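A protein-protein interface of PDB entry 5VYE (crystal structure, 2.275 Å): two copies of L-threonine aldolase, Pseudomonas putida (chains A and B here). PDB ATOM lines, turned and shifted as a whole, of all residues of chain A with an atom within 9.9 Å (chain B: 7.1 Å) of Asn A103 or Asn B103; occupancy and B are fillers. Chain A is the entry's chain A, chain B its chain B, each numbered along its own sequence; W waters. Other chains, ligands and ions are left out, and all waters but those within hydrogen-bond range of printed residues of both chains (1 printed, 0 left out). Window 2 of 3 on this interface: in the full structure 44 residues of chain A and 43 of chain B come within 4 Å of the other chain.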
ATOM      1  N   SER A  69      -0.159 -21.184  -9.290  1.00  0.00           N
ATOM      2  CA  SER A  69       0.201 -21.158 -10.691  1.00  0.00           C
ATOM      3  C   SER A  69       0.241 -22.577 -11.253  1.00  0.00           C
ATOM      4  O   SER A  69      -0.170 -22.806 -12.394  1.00  0.00           O
ATOM      5  CB  SER A  69       1.525 -20.431 -10.856  1.00  0.00           C
ATOM      6  OG  SER A  69       1.366 -19.025 -10.571  1.00  0.00           O
ATOM      7  N   LEU A  70       0.738 -23.537 -10.459  1.00  0.00           N
ATOM      8  CA  LEU A  70       0.796 -24.929 -10.886  1.00  0.00           C
ATOM      9  C   LEU A  70      -0.603 -25.515 -11.022  1.00  0.00           C
ATOM     10  O   LEU A  70      -0.882 -26.277 -11.960  1.00  0.00           O
ATOM     11  CB  LEU A  70       1.586 -25.745  -9.861  1.00  0.00           C
ATOM     12  CG  LEU A  70       3.072 -25.600  -9.846  1.00  0.00           C
ATOM     13  CD1 LEU A  70       3.628 -26.096  -8.524  1.00  0.00           C
ATOM     14  CD2 LEU A  70       3.726 -26.367 -11.019  1.00  0.00           C
ATOM     15  N   LEU A  72      -3.514 -23.937 -11.476  1.00  0.00           N
ATOM     16  CA  LEU A  72      -4.171 -23.399 -12.665  1.00  0.00           C
ATOM     17  C   LEU A  72      -3.582 -23.993 -13.952  1.00  0.00           C
ATOM     18  O   LEU A  72      -4.317 -24.300 -14.900  1.00  0.00           O
ATOM     19  CB  LEU A  72      -4.059 -21.886 -12.647  1.00  0.00           C
ATOM     20  CG  LEU A  72      -4.895 -21.239 -11.518  1.00  0.00           C
ATOM     21  CD1 LEU A  72      -4.664 -19.744 -11.496  1.00  0.00           C
ATOM     22  CD2 LEU A  72      -6.385 -21.503 -11.688  1.00  0.00           C
ATOM     23  N   ALA A  73      -2.279 -24.219 -13.987  1.00  0.00           N
ATOM     24  CA  ALA A  73      -1.673 -24.718 -15.225  1.00  0.00           C
ATOM     25  C   ALA A  73      -2.121 -26.138 -15.518  1.00  0.00           C
ATOM     26  O   ALA A  73      -2.223 -26.513 -16.678  1.00  0.00           O
ATOM     27  CB  ALA A  73      -0.157 -24.646 -15.162  1.00  0.00           C
ATOM     28  N   SER A  74      -2.441 -26.923 -14.498  1.00  0.00           N
ATOM     29  CA  SER A  74      -2.896 -28.287 -14.730  1.00  0.00           C
ATOM     30  C   SER A  74      -4.360 -28.329 -15.109  1.00  0.00           C
ATOM     31  O   SER A  74      -4.852 -29.382 -15.516  1.00  0.00           O
ATOM     32  CB  SER A  74      -2.668 -29.135 -13.475  1.00  0.00           C
ATOM     33  OG  SER A  74      -3.597 -28.795 -12.436  1.00  0.00           O
ATOM     34  N   CYS A  76      -6.020 -26.249 -17.362  1.00  0.00           N
ATOM     35  CA  CYS A  76      -6.343 -25.896 -18.734  1.00  0.00           C
ATOM     36  C   CYS A  76      -5.040 -25.741 -19.506  1.00  0.00           C
ATOM     37  O   CYS A  76      -3.948 -25.796 -18.939  1.00  0.00           O
ATOM     38  CB  CYS A  76      -7.158 -24.623 -18.828  1.00  0.00           C
ATOM     39  SG  CYS A  76      -6.288 -23.151 -18.300  1.00  0.00           S
ATOM     40  N   GLN A  77      -5.183 -25.525 -20.808  1.00  0.00           N
ATOM     41  CA  GLN A  77      -4.070 -25.387 -21.720  1.00  0.00           C
ATOM     42  C   GLN A  77      -3.709 -23.927 -21.834  1.00  0.00           C
ATOM     43  O   GLN A  77      -4.469 -23.053 -21.421  1.00  0.00           O
ATOM     44  CB  GLN A  77      -4.437 -25.930 -23.083  1.00  0.00           C
ATOM     45  CG  GLN A  77      -4.938 -27.364 -23.015  1.00  0.00           C
ATOM     46  CD  GLN A  77      -3.810 -28.336 -23.060  1.00  0.00           C
ATOM     47  OE1 GLN A  77      -3.474 -28.895 -24.122  1.00  0.00           O
ATOM     48  NE2 GLN A  77      -3.201 -28.548 -21.910  1.00  0.00           N
ATOM     49  N   SER A  78      -2.533 -23.680 -22.408  1.00  0.00           N
ATOM     50  CA  SER A  78      -2.032 -22.329 -22.583  1.00  0.00           C
ATOM     51  C   SER A  78      -2.922 -21.497 -23.481  1.00  0.00           C
ATOM     52  O   SER A  78      -2.899 -20.253 -23.400  1.00  0.00           O
ATOM     53  CB  SER A  78      -0.642 -22.356 -23.211  1.00  0.00           C
ATOM     54  OG  SER A  78      -0.609 -22.924 -24.520  1.00  0.00           O
ATOM     55  N   TYR A  79      -3.608 -22.147 -24.420  1.00  0.00           N
ATOM     56  CA  TYR A  79      -4.489 -21.430 -25.337  1.00  0.00           C
ATOM     57  C   TYR A  79      -5.902 -21.349 -24.775  1.00  0.00           C
ATOM     58  O   TYR A  79      -6.813 -20.934 -25.484  1.00  0.00           O
ATOM     59  CB  TYR A  79      -4.473 -22.085 -26.730  1.00  0.00           C
ATOM     60  CG  TYR A  79      -4.647 -23.590 -26.704  1.00  0.00           C
ATOM     61  CD1 TYR A  79      -5.895 -24.183 -26.494  1.00  0.00           C
ATOM     62  CD2 TYR A  79      -3.562 -24.415 -26.867  1.00  0.00           C
ATOM     63  CE1 TYR A  79      -6.022 -25.553 -26.451  1.00  0.00           C
ATOM     64  CE2 TYR A  79      -3.693 -25.810 -26.846  1.00  0.00           C
ATOM     65  CZ  TYR A  79      -4.917 -26.356 -26.633  1.00  0.00           C
ATOM     66  OH  TYR A  79      -5.034 -27.725 -26.604  1.00  0.00           O
ATOM     67  N   HIS A  80      -6.079 -21.700 -23.498  1.00  0.00           N
ATOM     68  CA  HIS A  80      -7.317 -21.512 -22.753  1.00  0.00           C
ATOM     69  C   HIS A  80      -7.115 -20.372 -21.771  1.00  0.00           C
ATOM     70  O   HIS A  80      -5.988 -19.970 -21.503  1.00  0.00           O
ATOM     71  CB  HIS A  80      -7.678 -22.773 -21.964  1.00  0.00           C
ATOM     72  CG  HIS A  80      -8.092 -23.933 -22.812  1.00  0.00           C
ATOM     73  ND1 HIS A  80      -7.809 -25.241 -22.473  1.00  0.00           N
ATOM     74  CD2 HIS A  80      -8.783 -23.984 -23.973  1.00  0.00           C
ATOM     75  CE1 HIS A  80      -8.318 -26.046 -23.384  1.00  0.00           C
ATOM     76  NE2 HIS A  80      -8.906 -25.308 -24.309  1.00  0.00           N
ATOM     77  N   GLY A  96       3.269 -12.005 -12.680  1.00  0.00           N
ATOM     78  CA  GLY A  96       3.042 -12.757 -13.894  1.00  0.00           C
ATOM     79  C   GLY A  96       3.368 -14.236 -13.832  1.00  0.00           C
ATOM     80  O   GLY A  96       3.599 -14.855 -14.884  1.00  0.00           O
ATOM     81  N   ALA A  97       3.391 -14.824 -12.632  1.00  0.00           N
ATOM     82  CA  ALA A  97       3.723 -16.219 -12.492  1.00  0.00           C
ATOM     83  C   ALA A  97       2.680 -17.102 -13.158  1.00  0.00           C
ATOM     84  O   ALA A  97       3.052 -18.105 -13.797  1.00  0.00           O
ATOM     85  CB  ALA A  97       3.884 -16.587 -11.009  1.00  0.00           C
ATOM     86  N   PRO A  98       1.385 -16.828 -13.023  1.00  0.00           N
ATOM     87  CA  PRO A  98       0.423 -17.756 -13.658  1.00  0.00           C
ATOM     88  C   PRO A  98       0.720 -17.961 -15.141  1.00  0.00           C
ATOM     89  O   PRO A  98       0.739 -19.095 -15.640  1.00  0.00           O
ATOM     90  CB  PRO A  98      -0.936 -17.079 -13.409  1.00  0.00           C
ATOM     91  CG  PRO A  98      -0.727 -16.386 -12.042  1.00  0.00           C
ATOM     92  CD  PRO A  98       0.689 -15.804 -12.192  1.00  0.00           C
ATOM     93  N   GLU A  99       1.050 -16.870 -15.818  1.00  0.00           N
ATOM     94  CA  GLU A  99       1.261 -16.864 -17.263  1.00  0.00           C
ATOM     95  C   GLU A  99       2.574 -17.548 -17.648  1.00  0.00           C
ATOM     96  O   GLU A  99       2.659 -18.206 -18.692  1.00  0.00           O
ATOM     97  CB  GLU A  99       1.236 -15.416 -17.758  1.00  0.00           C
ATOM     98  CG  GLU A  99      -0.150 -14.813 -17.790  1.00  0.00           C
ATOM     99  CD  GLU A  99      -0.507 -13.989 -16.543  1.00  0.00           C
ATOM    100  OE1 GLU A  99       0.118 -14.162 -15.477  1.00  0.00           O
ATOM    101  OE2 GLU A  99      -1.409 -13.131 -16.647  1.00  0.00           O
ATOM    102  N   PHE A 100       3.600 -17.394 -16.810  1.00  0.00           N
ATOM    103  CA  PHE A 100       4.850 -18.123 -16.965  1.00  0.00           C
ATOM    104  C   PHE A 100       4.628 -19.627 -16.806  1.00  0.00           C
ATOM    105  O   PHE A 100       5.092 -20.420 -17.625  1.00  0.00           O
ATOM    106  CB  PHE A 100       5.854 -17.575 -15.935  1.00  0.00           C
ATOM    107  CG  PHE A 100       7.158 -18.336 -15.866  1.00  0.00           C
ATOM    108  CD1 PHE A 100       8.151 -18.121 -16.793  1.00  0.00           C
ATOM    109  CD2 PHE A 100       7.389 -19.239 -14.835  1.00  0.00           C
ATOM    110  CE1 PHE A 100       9.357 -18.834 -16.733  1.00  0.00           C
ATOM    111  CE2 PHE A 100       8.556 -19.971 -14.784  1.00  0.00           C
ATOM    112  CZ  PHE A 100       9.562 -19.759 -15.739  1.00  0.00           C
ATOM    113  N   PHE A 101       3.904 -20.034 -15.762  1.00  0.00           N
ATOM    114  CA  PHE A 101       3.735 -21.452 -15.461  1.00  0.00           C
ATOM    115  C   PHE A 101       2.824 -22.128 -16.464  1.00  0.00           C
ATOM    116  O   PHE A 101       2.906 -23.340 -16.623  1.00  0.00           O
ATOM    117  CB  PHE A 101       3.118 -21.660 -14.072  1.00  0.00           C
ATOM    118  CG  PHE A 101       4.114 -21.683 -12.935  1.00  0.00           C
ATOM    119  CD1 PHE A 101       4.680 -20.499 -12.467  1.00  0.00           C
ATOM    120  CD2 PHE A 101       4.433 -22.879 -12.287  1.00  0.00           C
ATOM    121  CE1 PHE A 101       5.607 -20.516 -11.429  1.00  0.00           C
ATOM    122  CE2 PHE A 101       5.323 -22.887 -11.208  1.00  0.00           C
ATOM    123  CZ  PHE A 101       5.904 -21.703 -10.787  1.00  0.00           C
ATOM    124  N   SER A 102       1.866 -21.386 -17.036  1.00  0.00           N
ATOM    125  CA  SER A 102       0.938 -21.923 -18.018  1.00  0.00           C
ATOM    126  C   SER A 102       1.381 -21.718 -19.461  1.00  0.00           C
ATOM    127  O   SER A 102       0.706 -22.238 -20.355  1.00  0.00           O
ATOM    128  CB  SER A 102      -0.436 -21.254 -17.851  1.00  0.00           C
ATOM    129  OG  SER A 102      -0.360 -19.906 -18.298  1.00  0.00           O
ATOM    130  N   ASN A 103       2.479 -20.970 -19.697  1.00  0.00           N
ATOM    131  CA  ASN A 103       3.023 -20.650 -21.033  1.00  0.00           C
ATOM    132  C   ASN A 103       2.023 -19.840 -21.861  1.00  0.00           C
ATOM    133  O   ASN A 103       1.901 -20.030 -23.071  1.00  0.00           O
ATOM    134  CB  ASN A 103       3.471 -21.919 -21.781  1.00  0.00           C
ATOM    135  CG  ASN A 103       4.504 -21.629 -22.997  1.00  0.00           C
ATOM    136  OD1 ASN A 103       5.229 -20.568 -23.073  1.00  0.00           O
ATOM    137  ND2 ASN A 103       4.582 -22.622 -23.933  1.00  0.00           N
ATOM    138  N   GLY A 104       1.301 -18.929 -21.196  1.00  0.00           N
ATOM    139  CA  GLY A 104       0.447 -17.991 -21.888  1.00  0.00           C
ATOM    140  C   GLY A 104      -1.051 -18.039 -21.678  1.00  0.00           C
ATOM    141  O   GLY A 104      -1.774 -17.438 -22.475  1.00  0.00           O
ATOM    142  N   SER A 105      -1.560 -18.728 -20.650  1.00  0.00           N
ATOM    143  CA  SER A 105      -2.995 -18.722 -20.431  1.00  0.00           C
ATOM    144  C   SER A 105      -3.397 -17.322 -20.001  1.00  0.00           C
ATOM    145  O   SER A 105      -2.888 -16.821 -18.991  1.00  0.00           O
ATOM    146  CB  SER A 105      -3.393 -19.738 -19.368  1.00  0.00           C
ATOM    147  OG  SER A 105      -3.386 -21.063 -19.855  1.00  0.00           O
ATOM    148  N   LYS A 106      -4.304 -16.693 -20.750  1.00  0.00           N
ATOM    149  CA  LYS A 106      -4.789 -15.352 -20.385  1.00  0.00           C
ATOM    150  C   LYS A 106      -5.629 -15.391 -19.097  1.00  0.00           C
ATOM    151  O   LYS A 106      -6.550 -16.203 -18.965  1.00  0.00           O
ATOM    152  CB  LYS A 106      -5.640 -14.761 -21.525  1.00  0.00           C
ATOM    153  CG  LYS A 106      -4.884 -13.812 -22.454  1.00  0.00           C
ATOM    154  CD  LYS A 106      -5.783 -13.035 -23.388  1.00  0.00           C
ATOM    155  CE  LYS A 106      -5.893 -11.578 -22.966  1.00  0.00           C
ATOM    156  NZ  LYS A 106      -4.574 -10.854 -23.056  1.00  0.00           N
ATOM    157  N   LEU A 107      -5.298 -14.533 -18.136  1.00  0.00           N
ATOM    158  CA  LEU A 107      -6.185 -14.261 -17.005  1.00  0.00           C
ATOM    159  C   LEU A 107      -7.185 -13.160 -17.395  1.00  0.00           C
ATOM    160  O   LEU A 107      -6.795 -12.011 -17.598  1.00  0.00           O
ATOM    161  CB  LEU A 107      -5.380 -13.838 -15.782  1.00  0.00           C
ATOM    162  CG  LEU A 107      -4.406 -14.778 -15.074  1.00  0.00           C
ATOM    163  CD1 LEU A 107      -4.102 -14.134 -13.760  1.00  0.00           C
ATOM    164  CD2 LEU A 107      -5.019 -16.119 -14.852  1.00  0.00           C
ATOM    165  N   PRO A 135      -8.786 -16.625 -26.248  1.00  0.00           N
ATOM    166  CA  PRO A 135      -8.577 -17.876 -25.497  1.00  0.00           C
ATOM    167  C   PRO A 135      -9.847 -18.289 -24.766  1.00  0.00           C
ATOM    168  O   PRO A 135     -10.456 -17.501 -24.041  1.00  0.00           O
ATOM    169  CB  PRO A 135      -7.451 -17.520 -24.518  1.00  0.00           C
ATOM    170  CG  PRO A 135      -6.871 -16.265 -24.982  1.00  0.00           C
ATOM    171  CD  PRO A 135      -7.979 -15.528 -25.691  1.00  0.00           C
ATOM    172  N   ARG A 230       4.784 -32.295 -13.027  1.00  0.00           N
ATOM    173  CA  ARG A 230       4.679 -30.854 -13.224  1.00  0.00           C
ATOM    174  C   ARG A 230       5.431 -30.101 -12.150  1.00  0.00           C
ATOM    175  O   ARG A 230       6.253 -29.225 -12.452  1.00  0.00           O
ATOM    176  CB  ARG A 230       3.211 -30.441 -13.281  1.00  0.00           C
ATOM    177  CG  ARG A 230       3.025 -29.028 -13.775  1.00  0.00           C
ATOM    178  CD  ARG A 230       1.591 -28.599 -13.654  1.00  0.00           C
ATOM    179  NE  ARG A 230       0.782 -29.222 -14.674  1.00  0.00           N
ATOM    180  CZ  ARG A 230       0.713 -28.795 -15.943  1.00  0.00           C
ATOM    181  NH1 ARG A 230       1.396 -27.749 -16.352  1.00  0.00           N
ATOM    182  NH2 ARG A 230      -0.044 -29.435 -16.801  1.00  0.00           N
ATOM    183  N   GLN A 233       9.307 -30.543 -12.605  1.00  0.00           N
ATOM    184  CA  GLN A 233       9.856 -29.702 -13.662  1.00  0.00           C
ATOM    185  C   GLN A 233       9.800 -28.228 -13.256  1.00  0.00           C
ATOM    186  O   GLN A 233      10.654 -27.415 -13.671  1.00  0.00           O
ATOM    187  CB  GLN A 233       9.100 -29.961 -14.982  1.00  0.00           C
ATOM    188  CG  GLN A 233       9.459 -29.013 -16.081  1.00  0.00           C
ATOM    189  CD  GLN A 233       8.790 -29.292 -17.376  1.00  0.00           C
ATOM    190  OE1 GLN A 233       7.562 -29.252 -17.479  1.00  0.00           O
ATOM    191  NE2 GLN A 233       9.594 -29.513 -18.419  1.00  0.00           N
ATOM    192  N   ALA B  73      18.799 -19.698 -17.146  1.00  0.00           N
ATOM    193  CA  ALA B  73      17.880 -18.919 -17.955  1.00  0.00           C
ATOM    194  C   ALA B  73      18.259 -17.453 -17.983  1.00  0.00           C
ATOM    195  O   ALA B  73      17.935 -16.739 -18.956  1.00  0.00           O
ATOM    196  CB  ALA B  73      16.481 -19.095 -17.411  1.00  0.00           C
ATOM    197  N   GLN B  77      19.350 -16.601 -24.064  1.00  0.00           N
ATOM    198  CA  GLN B  77      17.980 -16.584 -24.540  1.00  0.00           C
ATOM    199  C   GLN B  77      17.518 -18.010 -24.848  1.00  0.00           C
ATOM    200  O   GLN B  77      18.333 -18.944 -24.953  1.00  0.00           O
ATOM    201  CB  GLN B  77      17.889 -15.702 -25.793  1.00  0.00           C
ATOM    202  CG  GLN B  77      18.456 -14.307 -25.568  1.00  0.00           C
ATOM    203  CD  GLN B  77      17.487 -13.412 -24.838  1.00  0.00           C
ATOM    204  OE1 GLN B  77      17.303 -13.504 -23.633  1.00  0.00           O
ATOM    205  NE2 GLN B  77      16.834 -12.560 -25.587  1.00  0.00           N
ATOM    206  N   SER B  78      16.201 -18.159 -25.016  1.00  0.00           N
ATOM    207  CA  SER B  78      15.625 -19.445 -25.390  1.00  0.00           C
ATOM    208  C   SER B  78      16.163 -19.965 -26.714  1.00  0.00           C
ATOM    209  O   SER B  78      16.213 -21.191 -26.919  1.00  0.00           O
ATOM    210  CB  SER B  78      14.123 -19.358 -25.496  1.00  0.00           C
ATOM    211  OG  SER B  78      13.721 -18.540 -26.556  1.00  0.00           O
ATOM    212  N   TYR B  79      16.613 -19.070 -27.590  1.00  0.00           N
ATOM    213  CA  TYR B  79      17.182 -19.458 -28.882  1.00  0.00           C
ATOM    214  C   TYR B  79      18.694 -19.601 -28.815  1.00  0.00           C
ATOM    215  O   TYR B  79      19.326 -19.798 -29.847  1.00  0.00           O
ATOM    216  CB  TYR B  79      16.782 -18.455 -29.985  1.00  0.00           C
ATOM    217  CG  TYR B  79      16.976 -17.016 -29.618  1.00  0.00           C
ATOM    218  CD1 TYR B  79      18.227 -16.390 -29.718  1.00  0.00           C
ATOM    219  CD2 TYR B  79      15.925 -16.283 -29.184  1.00  0.00           C
ATOM    220  CE1 TYR B  79      18.373 -15.071 -29.418  1.00  0.00           C
ATOM    221  CE2 TYR B  79      16.067 -14.958 -28.868  1.00  0.00           C
ATOM    222  CZ  TYR B  79      17.284 -14.345 -28.997  1.00  0.00           C
ATOM    223  OH  TYR B  79      17.434 -13.011 -28.671  1.00  0.00           O
ATOM    224  N   ALA B  97      13.549 -29.331 -16.106  1.00  0.00           N
ATOM    225  CA  ALA B  97      13.352 -27.996 -15.552  1.00  0.00           C
ATOM    226  C   ALA B  97      14.129 -26.926 -16.303  1.00  0.00           C
ATOM    227  O   ALA B  97      13.612 -25.802 -16.425  1.00  0.00           O
ATOM    228  CB  ALA B  97      13.744 -27.961 -14.074  1.00  0.00           C
ATOM    229  N   PRO B  98      15.366 -27.157 -16.752  1.00  0.00           N
ATOM    230  CA  PRO B  98      16.078 -26.066 -17.415  1.00  0.00           C
ATOM    231  C   PRO B  98      15.333 -25.586 -18.642  1.00  0.00           C
ATOM    232  O   PRO B  98      15.175 -24.374 -18.838  1.00  0.00           O
ATOM    233  CB  PRO B  98      17.453 -26.700 -17.726  1.00  0.00           C
ATOM    234  CG  PRO B  98      17.686 -27.579 -16.528  1.00  0.00           C
ATOM    235  CD  PRO B  98      16.296 -28.233 -16.351  1.00  0.00           C
ATOM    236  N   GLU B  99      14.773 -26.515 -19.411  1.00  0.00           N
ATOM    237  CA  GLU B  99      14.087 -26.149 -20.645  1.00  0.00           C
ATOM    238  C   GLU B  99      12.771 -25.434 -20.356  1.00  0.00           C
ATOM    239  O   GLU B  99      12.421 -24.476 -21.040  1.00  0.00           O
ATOM    240  CB  GLU B  99      13.864 -27.395 -21.490  1.00  0.00           C
ATOM    241  CG  GLU B  99      15.115 -27.972 -22.142  1.00  0.00           C
ATOM    242  CD  GLU B  99      15.851 -28.983 -21.256  1.00  0.00           C
ATOM    243  OE1 GLU B  99      15.569 -29.000 -20.041  1.00  0.00           O
ATOM    244  OE2 GLU B  99      16.665 -29.792 -21.788  1.00  0.00           O
ATOM    245  N   PHE B 100      12.056 -25.864 -19.318  1.00  0.00           N
ATOM    246  CA  PHE B 100      10.867 -25.153 -18.850  1.00  0.00           C
ATOM    247  C   PHE B 100      11.202 -23.731 -18.440  1.00  0.00           C
ATOM    248  O   PHE B 100      10.558 -22.797 -18.886  1.00  0.00           O
ATOM    249  CB  PHE B 100      10.271 -25.917 -17.677  1.00  0.00           C
ATOM    250  CG  PHE B 100       9.100 -25.254 -17.028  1.00  0.00           C
ATOM    251  CD1 PHE B 100       7.868 -25.290 -17.612  1.00  0.00           C
ATOM    252  CD2 PHE B 100       9.234 -24.658 -15.775  1.00  0.00           C
ATOM    253  CE1 PHE B 100       6.717 -24.691 -16.973  1.00  0.00           C
ATOM    254  CE2 PHE B 100       8.121 -24.047 -15.121  1.00  0.00           C
ATOM    255  CZ  PHE B 100       6.839 -24.086 -15.740  1.00  0.00           C
ATOM    256  N   PHE B 101      12.224 -23.545 -17.589  1.00  0.00           N
ATOM    257  CA  PHE B 101      12.522 -22.198 -17.079  1.00  0.00           C
ATOM    258  C   PHE B 101      13.072 -21.256 -18.139  1.00  0.00           C
ATOM    259  O   PHE B 101      12.916 -20.039 -17.995  1.00  0.00           O
ATOM    260  CB  PHE B 101      13.539 -22.247 -15.927  1.00  0.00           C
ATOM    261  CG  PHE B 101      12.927 -22.595 -14.616  1.00  0.00           C
ATOM    262  CD1 PHE B 101      12.576 -23.920 -14.335  1.00  0.00           C
ATOM    263  CD2 PHE B 101      12.711 -21.622 -13.650  1.00  0.00           C
ATOM    264  CE1 PHE B 101      11.990 -24.269 -13.106  1.00  0.00           C
ATOM    265  CE2 PHE B 101      12.205 -21.966 -12.375  1.00  0.00           C
ATOM    266  CZ  PHE B 101      11.835 -23.278 -12.105  1.00  0.00           C
ATOM    267  N   SER B 102      13.799 -21.781 -19.143  1.00  0.00           N
ATOM    268  CA  SER B 102      14.355 -20.967 -20.205  1.00  0.00           C
ATOM    269  C   SER B 102      13.425 -20.813 -21.402  1.00  0.00           C
ATOM    270  O   SER B 102      13.759 -20.096 -22.329  1.00  0.00           O
ATOM    271  CB  SER B 102      15.676 -21.562 -20.723  1.00  0.00           C
ATOM    272  OG  SER B 102      15.518 -22.851 -21.330  1.00  0.00           O
ATOM    273  N   ASN B 103      12.324 -21.536 -21.452  1.00  0.00           N
ATOM    274  CA  ASN B 103      11.427 -21.526 -22.585  1.00  0.00           C
ATOM    275  C   ASN B 103      12.096 -22.091 -23.849  1.00  0.00           C
ATOM    276  O   ASN B 103      11.789 -21.655 -24.951  1.00  0.00           O
ATOM    277  CB  ASN B 103      10.881 -20.095 -22.813  1.00  0.00           C
ATOM    278  CG  ASN B 103       9.455 -19.993 -23.525  1.00  0.00           C
ATOM    279  OD1 ASN B 103       8.990 -18.802 -23.782  1.00  0.00           O
ATOM    280  ND2 ASN B 103       8.752 -21.138 -23.811  1.00  0.00           N
ATOM    281  N   GLY B 104      13.008 -23.069 -23.726  1.00  0.00           N
ATOM    282  CA  GLY B 104      13.466 -23.795 -24.891  1.00  0.00           C
ATOM    283  C   GLY B 104      14.946 -23.760 -25.208  1.00  0.00           C
ATOM    284  O   GLY B 104      15.352 -24.161 -26.305  1.00  0.00           O
ATOM    285  N   SER B 105      15.778 -23.278 -24.287  1.00  0.00           N
ATOM    286  CA  SER B 105      17.217 -23.407 -24.504  1.00  0.00           C
ATOM    287  C   SER B 105      17.583 -24.875 -24.552  1.00  0.00           C
ATOM    288  O   SER B 105      17.307 -25.615 -23.604  1.00  0.00           O
ATOM    289  CB  SER B 105      18.002 -22.678 -23.421  1.00  0.00           C
ATOM    290  OG  SER B 105      17.823 -21.296 -23.608  1.00  0.00           O
HETATM  291  O   HOH W   1       6.575 -20.412 -25.457  1.00  0.00           O
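Phe A100 touches Phe B101, but with the chains exchanged Phe A101 does not touch Phe B100 (4.1 Å).
Asn B103 touches its own counterpart, Asn A103.
Positions printed for both chains: 73, 77, 78, 79, 97, 98, 99, 100, 101, 102, 103, 104 and 105.
Among the printed residues, merely in contact across the chains: Gln A233 with Ala B97 (3.2 Å), Gln A233 with Phe B101 (3.5 Å), Gln A233 with Phe B100 (3.6 Å), Asn A103 with Asn B103 (3.6 Å) and Phe A100 with Phe B101 (3.96 Å).
Water W1 lies within hydrogen-bond range of OD1 of Asn A103 (2.7 Å) and ND2 of Asn B103 (2.8 Å).
Hydrophobic or aromatic side chains of chain A that line the printed part of chain B: Phe A100.
Printed residues of chain B that touch a printed residue of chain A: Ala B97, Phe B100, Phe B101 and Asn B103.
Hydrophobic or aromatic side chains of chain B that line the printed part of chain A: Ala B97, Phe B100 and Phe B101.
Along chain B the printed residues that touch a printed residue of chain A span positions 97 to 103.
Among the printed residues, 5 pairs touch across the chains.
Among the printed residues, no Asp or Glu carboxylate lies within 4 Å of a Lys or Arg side-chain nitrogen of the other chain.
Of the printed residues of chain B, Asn A103 touches Asn B103 (3.6 Å).
Of the printed residues of chain A, Asn B103 touches Asn A103.
No residue of chain A comes within 4 Å of Ser B78.
No residue of chain A comes within 4 Å of Ser B102.
No residue of chain A comes within 4 Å of Gly B104.
Of the printed residues of chain A, Phe B101 touches Phe A100 (3.96 Å) and Gln A233 (3.5 Å).
Of the printed residues of chain A, Ala B97 touches Gln A233 (3.2 Å).
Of the printed residues of chain B, Phe A100 touches Phe B101.
Printed residues of chain A within 4 Å of Phe B100: Gln A233 (3.6 Å).
Of the printed residues of chain B, Gln A233 touches Ala B97, Phe B100 and Phe B101.
The nearest residue of chain A that does not touch Asn B103 is Phe A100 (6.2 Å).
The nearest printed residue of chain A that does not touch Phe B100 is Phe A101 (4.1 Å).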
